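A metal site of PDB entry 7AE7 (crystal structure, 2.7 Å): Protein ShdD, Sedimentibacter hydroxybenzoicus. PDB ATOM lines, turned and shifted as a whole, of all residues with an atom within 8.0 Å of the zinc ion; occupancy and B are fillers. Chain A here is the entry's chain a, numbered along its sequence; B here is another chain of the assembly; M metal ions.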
ATOM      1  N   LYS A   2      21.583  28.768  -4.711  1.00  0.00           N
ATOM      2  CA  LYS A   2      20.449  29.689  -4.681  1.00  0.00           C
ATOM      3  C   LYS A   2      19.231  29.032  -5.312  1.00  0.00           C
ATOM      4  O   LYS A   2      19.339  28.120  -6.139  1.00  0.00           O
ATOM      5  CB  LYS A   2      20.775  31.001  -5.415  1.00  0.00           C
ATOM      6  N   CYS A   3      18.063  29.504  -4.888  1.00  0.00           N
ATOM      7  CA  CYS A   3      16.797  28.979  -5.386  1.00  0.00           C
ATOM      8  C   CYS A   3      16.584  29.411  -6.841  1.00  0.00           C
ATOM      9  O   CYS A   3      16.683  30.597  -7.165  1.00  0.00           O
ATOM     10  CB  CYS A   3      15.658  29.464  -4.499  1.00  0.00           C
ATOM     11  SG  CYS A   3      13.989  29.257  -5.151  1.00  0.00           S
ATOM     12  N   HIS A   4      16.301  28.441  -7.713  1.00  0.00           N
ATOM     13  CA  HIS A   4      16.148  28.736  -9.140  1.00  0.00           C
ATOM     14  C   HIS A   4      14.908  29.568  -9.432  1.00  0.00           C
ATOM     15  O   HIS A   4      14.812  30.144 -10.520  1.00  0.00           O
ATOM     16  CB  HIS A   4      16.089  27.436  -9.956  1.00  0.00           C
ATOM     17  CG  HIS A   4      17.188  26.474  -9.633  1.00  0.00           C
ATOM     18  ND1 HIS A   4      18.383  26.447 -10.329  1.00  0.00           N
ATOM     19  CD2 HIS A   4      17.267  25.493  -8.701  1.00  0.00           C
ATOM     20  CE1 HIS A   4      19.153  25.487  -9.835  1.00  0.00           C
ATOM     21  NE2 HIS A   4      18.498  24.889  -8.851  1.00  0.00           N
ATOM     22  N   ARG A   5      13.970  29.656  -8.494  1.00  0.00           N
ATOM     23  CA  ARG A   5      12.743  30.408  -8.724  1.00  0.00           C
ATOM     24  C   ARG A   5      12.804  31.834  -8.209  1.00  0.00           C
ATOM     25  O   ARG A   5      12.480  32.775  -8.943  1.00  0.00           O
ATOM     26  CB  ARG A   5      11.545  29.681  -8.108  1.00  0.00           C
ATOM     27  CG  ARG A   5      10.239  30.411  -8.330  1.00  0.00           C
ATOM     28  CD  ARG A   5       9.055  29.474  -8.253  1.00  0.00           C
ATOM     29  NE  ARG A   5       8.726  29.132  -6.873  1.00  0.00           N
ATOM     30  CZ  ARG A   5       7.691  28.395  -6.509  1.00  0.00           C
ATOM     31  NH1 ARG A   5       6.846  27.896  -7.401  1.00  0.00           N
ATOM     32  NH2 ARG A   5       7.492  28.149  -5.225  1.00  0.00           N
ATOM     33  N   CYS A   6      13.208  32.028  -6.953  1.00  0.00           N
ATOM     34  CA  CYS A   6      13.181  33.348  -6.338  1.00  0.00           C
ATOM     35  C   CYS A   6      14.564  33.919  -6.059  1.00  0.00           C
ATOM     36  O   CYS A   6      14.665  35.089  -5.676  1.00  0.00           O
ATOM     37  CB  CYS A   6      12.369  33.315  -5.039  1.00  0.00           C
ATOM     38  SG  CYS A   6      13.249  32.619  -3.630  1.00  0.00           S
ATOM     39  N   GLY A   7      15.628  33.133  -6.224  1.00  0.00           N
ATOM     40  CA  GLY A   7      16.979  33.633  -6.082  1.00  0.00           C
ATOM     41  C   GLY A   7      17.495  33.725  -4.665  1.00  0.00           C
ATOM     42  O   GLY A   7      18.649  34.111  -4.472  1.00  0.00           O
ATOM     43  N   SER A   8      16.675  33.379  -3.667  1.00  0.00           N
ATOM     44  CA  SER A   8      17.144  33.389  -2.292  1.00  0.00           C
ATOM     45  C   SER A   8      18.267  32.380  -2.095  1.00  0.00           C
ATOM     46  O   SER A   8      18.316  31.347  -2.768  1.00  0.00           O
ATOM     47  CB  SER A   8      15.988  33.091  -1.340  1.00  0.00           C
ATOM     48  OG  SER A   8      16.460  32.530  -0.128  1.00  0.00           O
ATOM     49  N   ASP A   9      19.183  32.689  -1.191  1.00  0.00           N
ATOM     50  CA  ASP A   9      20.233  31.750  -0.818  1.00  0.00           C
ATOM     51  C   ASP A   9      19.849  30.896   0.376  1.00  0.00           C
ATOM     52  O   ASP A   9      20.661  30.070   0.812  1.00  0.00           O
ATOM     53  CB  ASP A   9      21.550  32.497  -0.547  1.00  0.00           C
ATOM     54  CG  ASP A   9      21.440  33.522   0.572  1.00  0.00           C
ATOM     55  OD1 ASP A   9      20.389  33.570   1.248  1.00  0.00           O
ATOM     56  OD2 ASP A   9      22.417  34.268   0.781  1.00  0.00           O
ATOM     57  N   ASN A  10      18.637  31.060   0.900  1.00  0.00           N
ATOM     58  CA  ASN A  10      18.160  30.298   2.058  1.00  0.00           C
ATOM     59  C   ASN A  10      17.620  28.951   1.578  1.00  0.00           C
ATOM     60  O   ASN A  10      16.416  28.695   1.551  1.00  0.00           O
ATOM     61  CB  ASN A  10      17.118  31.099   2.825  1.00  0.00           C
ATOM     62  CG  ASN A  10      16.901  30.595   4.230  1.00  0.00           C
ATOM     63  OD1 ASN A  10      17.707  29.820   4.751  1.00  0.00           O
ATOM     64  ND2 ASN A  10      15.832  31.039   4.865  1.00  0.00           N
ATOM     65  N   VAL A  11      18.550  28.077   1.201  1.00  0.00           N
ATOM     66  CA  VAL A  11      18.247  26.780   0.608  1.00  0.00           C
ATOM     67  C   VAL A  11      18.820  25.700   1.519  1.00  0.00           C
ATOM     68  O   VAL A  11      19.973  25.804   1.951  1.00  0.00           O
ATOM     69  CB  VAL A  11      18.817  26.659  -0.809  1.00  0.00           C
ATOM     70  CG1 VAL A  11      18.538  25.286  -1.394  1.00  0.00           C
ATOM     71  CG2 VAL A  11      18.276  27.757  -1.705  1.00  0.00           C
ATOM     72  N   VAL A  27      15.246  22.455  -1.070  1.00  0.00           N
ATOM     73  CA  VAL A  27      14.048  23.280  -0.954  1.00  0.00           C
ATOM     74  C   VAL A  27      14.455  24.694  -0.555  1.00  0.00           C
ATOM     75  O   VAL A  27      15.415  24.884   0.212  1.00  0.00           O
ATOM     76  CB  VAL A  27      13.049  22.680   0.057  1.00  0.00           C
ATOM     77  CG1 VAL A  27      13.686  22.573   1.445  1.00  0.00           C
ATOM     78  CG2 VAL A  27      11.757  23.499   0.118  1.00  0.00           C
ATOM     79  N   CYS A  28      13.752  25.681  -1.090  1.00  0.00           N
ATOM     80  CA  CYS A  28      13.944  27.074  -0.707  1.00  0.00           C
ATOM     81  C   CYS A  28      13.064  27.399   0.487  1.00  0.00           C
ATOM     82  O   CYS A  28      11.855  27.151   0.463  1.00  0.00           O
ATOM     83  CB  CYS A  28      13.608  27.993  -1.883  1.00  0.00           C
ATOM     84  SG  CYS A  28      13.372  29.715  -1.410  1.00  0.00           S
ATOM     85  N   GLU A  29      13.671  27.943   1.544  1.00  0.00           N
ATOM     86  CA  GLU A  29      12.942  28.264   2.764  1.00  0.00           C
ATOM     87  C   GLU A  29      12.066  29.493   2.629  1.00  0.00           C
ATOM     88  O   GLU A  29      11.287  29.785   3.547  1.00  0.00           O
ATOM     89  CB  GLU A  29      13.920  28.433   3.927  1.00  0.00           C
ATOM     90  CG  GLU A  29      14.666  27.169   4.295  1.00  0.00           C
ATOM     91  CD  GLU A  29      13.845  26.250   5.188  1.00  0.00           C
ATOM     92  OE1 GLU A  29      13.717  26.559   6.397  1.00  0.00           O
ATOM     93  OE2 GLU A  29      13.352  25.219   4.694  1.00  0.00           O
ATOM     94  N   LYS A  30      12.162  30.229   1.526  1.00  0.00           N
ATOM     95  CA  LYS A  30      11.387  31.440   1.330  1.00  0.00           C
ATOM     96  C   LYS A  30      10.162  31.245   0.454  1.00  0.00           C
ATOM     97  O   LYS A  30       9.108  31.831   0.743  1.00  0.00           O
ATOM     98  CB  LYS A  30      12.267  32.545   0.723  1.00  0.00           C
ATOM     99  CG  LYS A  30      11.620  33.911   0.729  1.00  0.00           C
ATOM    100  CD  LYS A  30      11.996  34.685  -0.510  1.00  0.00           C
ATOM    101  CE  LYS A  30      11.976  36.174  -0.229  1.00  0.00           C
ATOM    102  NZ  LYS A  30      13.134  36.847  -0.882  1.00  0.00           N
ATOM    103  N   CYS A  31      10.251  30.446  -0.614  1.00  0.00           N
ATOM    104  CA  CYS A  31       9.133  30.264  -1.521  1.00  0.00           C
ATOM    105  C   CYS A  31       8.726  28.804  -1.715  1.00  0.00           C
ATOM    106  O   CYS A  31       7.831  28.540  -2.533  1.00  0.00           O
ATOM    107  CB  CYS A  31       9.450  30.890  -2.887  1.00  0.00           C
ATOM    108  SG  CYS A  31      10.487  29.881  -3.953  1.00  0.00           S
ATOM    109  N   CYS A  32       9.344  27.867  -1.006  1.00  0.00           N
ATOM    110  CA  CYS A  32       9.006  26.442  -0.971  1.00  0.00           C
ATOM    111  C   CYS A  32       9.326  25.708  -2.262  1.00  0.00           C
ATOM    112  O   CYS A  32       8.938  24.546  -2.416  1.00  0.00           O
ATOM    113  CB  CYS A  32       7.525  26.200  -0.638  1.00  0.00           C
ATOM    114  SG  CYS A  32       6.945  27.046   0.839  1.00  0.00           S
ATOM    115  N   TYR A  33      10.023  26.335  -3.211  1.00  0.00           N
ATOM    116  CA  TYR A  33      10.424  25.624  -4.416  1.00  0.00           C
ATOM    117  C   TYR A  33      11.412  24.514  -4.056  1.00  0.00           C
ATOM    118  O   TYR A  33      12.321  24.715  -3.247  1.00  0.00           O
ATOM    119  CB  TYR A  33      11.058  26.584  -5.425  1.00  0.00           C
ATOM    120  CG  TYR A  33      11.378  25.929  -6.753  1.00  0.00           C
ATOM    121  CD1 TYR A  33      10.370  25.660  -7.664  1.00  0.00           C
ATOM    122  CD2 TYR A  33      12.681  25.583  -7.084  1.00  0.00           C
ATOM    123  CE1 TYR A  33      10.655  25.066  -8.884  1.00  0.00           C
ATOM    124  CE2 TYR A  33      12.964  24.984  -8.295  1.00  0.00           C
ATOM    125  CZ  TYR A  33      11.952  24.730  -9.188  1.00  0.00           C
ATOM    126  OH  TYR A  33      12.243  24.136 -10.395  1.00  0.00           O
ATOM    127  N   SER A  34      11.212  23.343  -4.643  1.00  0.00           N
ATOM    128  CA  SER A  34      12.065  22.197  -4.375  1.00  0.00           C
ATOM    129  C   SER A  34      12.518  21.583  -5.691  1.00  0.00           C
ATOM    130  O   SER A  34      11.875  21.742  -6.739  1.00  0.00           O
ATOM    131  CB  SER A  34      11.355  21.128  -3.520  1.00  0.00           C
ATOM    132  OG  SER A  34      10.039  20.889  -3.975  1.00  0.00           O
ATOM    133  N   TRP A  35      13.650  20.886  -5.633  1.00  0.00           N
ATOM    134  CA  TRP A  35      14.212  20.267  -6.839  1.00  0.00           C
ATOM    135  C   TRP A  35      15.250  19.219  -6.447  1.00  0.00           C
ATOM    136  O   TRP A  35      15.839  19.268  -5.365  1.00  0.00           O
ATOM    137  CB  TRP A  35      14.828  21.322  -7.764  1.00  0.00           C
ATOM    138  CG  TRP A  35      16.109  21.909  -7.263  1.00  0.00           C
ATOM    139  CD1 TRP A  35      17.378  21.492  -7.547  1.00  0.00           C
ATOM    140  CD2 TRP A  35      16.253  23.034  -6.378  1.00  0.00           C
ATOM    141  NE1 TRP A  35      18.298  22.277  -6.900  1.00  0.00           N
ATOM    142  CE2 TRP A  35      17.638  23.232  -6.175  1.00  0.00           C
ATOM    143  CE3 TRP A  35      15.348  23.885  -5.743  1.00  0.00           C
ATOM    144  CZ2 TRP A  35      18.124  24.247  -5.367  1.00  0.00           C
ATOM    145  CZ3 TRP A  35      15.839  24.892  -4.938  1.00  0.00           C
ATOM    146  CH2 TRP A  35      17.221  25.071  -4.758  1.00  0.00           C
ATOM    147  N   LEU A  49       9.903  34.407  -9.112  1.00  0.00           N
ATOM    148  CA  LEU A  49       9.304  35.150  -8.018  1.00  0.00           C
ATOM    149  C   LEU A  49      10.338  36.074  -7.379  1.00  0.00           C
ATOM    150  O   LEU A  49      11.544  35.884  -7.503  1.00  0.00           O
ATOM    151  CB  LEU A  49       8.717  34.215  -6.953  1.00  0.00           C
ATOM    152  CG  LEU A  49       7.558  33.328  -7.399  1.00  0.00           C
ATOM    153  CD1 LEU A  49       7.246  32.263  -6.353  1.00  0.00           C
ATOM    154  CD2 LEU A  49       6.320  34.173  -7.684  1.00  0.00           C
ATOM    155  N   ASP A  50       9.823  37.080  -6.680  1.00  0.00           N
ATOM    156  CA  ASP A  50      10.639  37.957  -5.840  1.00  0.00           C
ATOM    157  C   ASP A  50       9.833  38.300  -4.588  1.00  0.00           C
ATOM    158  O   ASP A  50       8.729  37.785  -4.381  1.00  0.00           O
ATOM    159  CB  ASP A  50      11.071  39.224  -6.591  1.00  0.00           C
ATOM    160  CG  ASP A  50       9.910  39.949  -7.240  1.00  0.00           C
ATOM    161  OD1 ASP A  50       9.019  40.430  -6.505  1.00  0.00           O
ATOM    162  OD2 ASP A  50       9.901  40.064  -8.484  1.00  0.00           O
ATOM    163  N   ILE A  54       5.764  37.799  -3.881  1.00  0.00           N
ATOM    164  CA  ILE A  54       5.261  36.977  -2.784  1.00  0.00           C
ATOM    165  C   ILE A  54       4.357  37.807  -1.872  1.00  0.00           C
ATOM    166  O   ILE A  54       3.274  37.359  -1.474  1.00  0.00           O
ATOM    167  CB  ILE A  54       6.424  36.354  -1.998  1.00  0.00           C
ATOM    168  CG1 ILE A  54       7.183  35.354  -2.880  1.00  0.00           C
ATOM    169  CG2 ILE A  54       5.913  35.657  -0.741  1.00  0.00           C
ATOM    170  CD1 ILE A  54       8.512  34.922  -2.294  1.00  0.00           C
ATOM    171  N   VAL B 272       3.806  29.382  -0.100  1.00  0.00           N
ATOM    172  CA  VAL B 272       3.649  29.383  -1.549  1.00  0.00           C
ATOM    173  C   VAL B 272       3.440  27.954  -2.036  1.00  0.00           C
ATOM    174  O   VAL B 272       4.281  27.082  -1.816  1.00  0.00           O
ATOM    175  CB  VAL B 272       4.848  30.037  -2.240  1.00  0.00           C
ATOM    176  CG1 VAL B 272       4.636  30.099  -3.747  1.00  0.00           C
ATOM    177  CG2 VAL B 272       5.082  31.430  -1.688  1.00  0.00           C
HETATM  178 ZN    ZN M   1      12.739  30.370  -3.547  1.00  0.00          ZN
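The side-chain sulfur of Cys 3 sits close to the backbone NH of Arg 5 (3.4 Å). SG of Cys 31 lies close to N of Tyr 33 (3.7 Å). O of Tyr 33 sits at hydrogen-bond distance from N of Cys 28 (2.8 Å). O of Cys 31 is in hydrogen-bond range of NH2 of Arg 5 (2.7 Å). The side-chain sulfur of Cys 28 sits close to the backbone NH of Lys 30, 3.2 Å away. The side-chain sulfur of Cys 6 sits close to the backbone NH of Ser 8 (3.5 Å). O of Ser 8 lies within hydrogen-bond range of N of Cys 3, 2.8 Å away.
The nearest printed residue that does not touch the zinc ion is Tyr 33 (4.5 Å).
The zinc ion is bound by SG of Cys 6 (2.3 Å), SG of Cys 3 (2.3 Å), SG of Cys 28 (2.3 Å) and SG of Cys 31 (2.3 Å).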
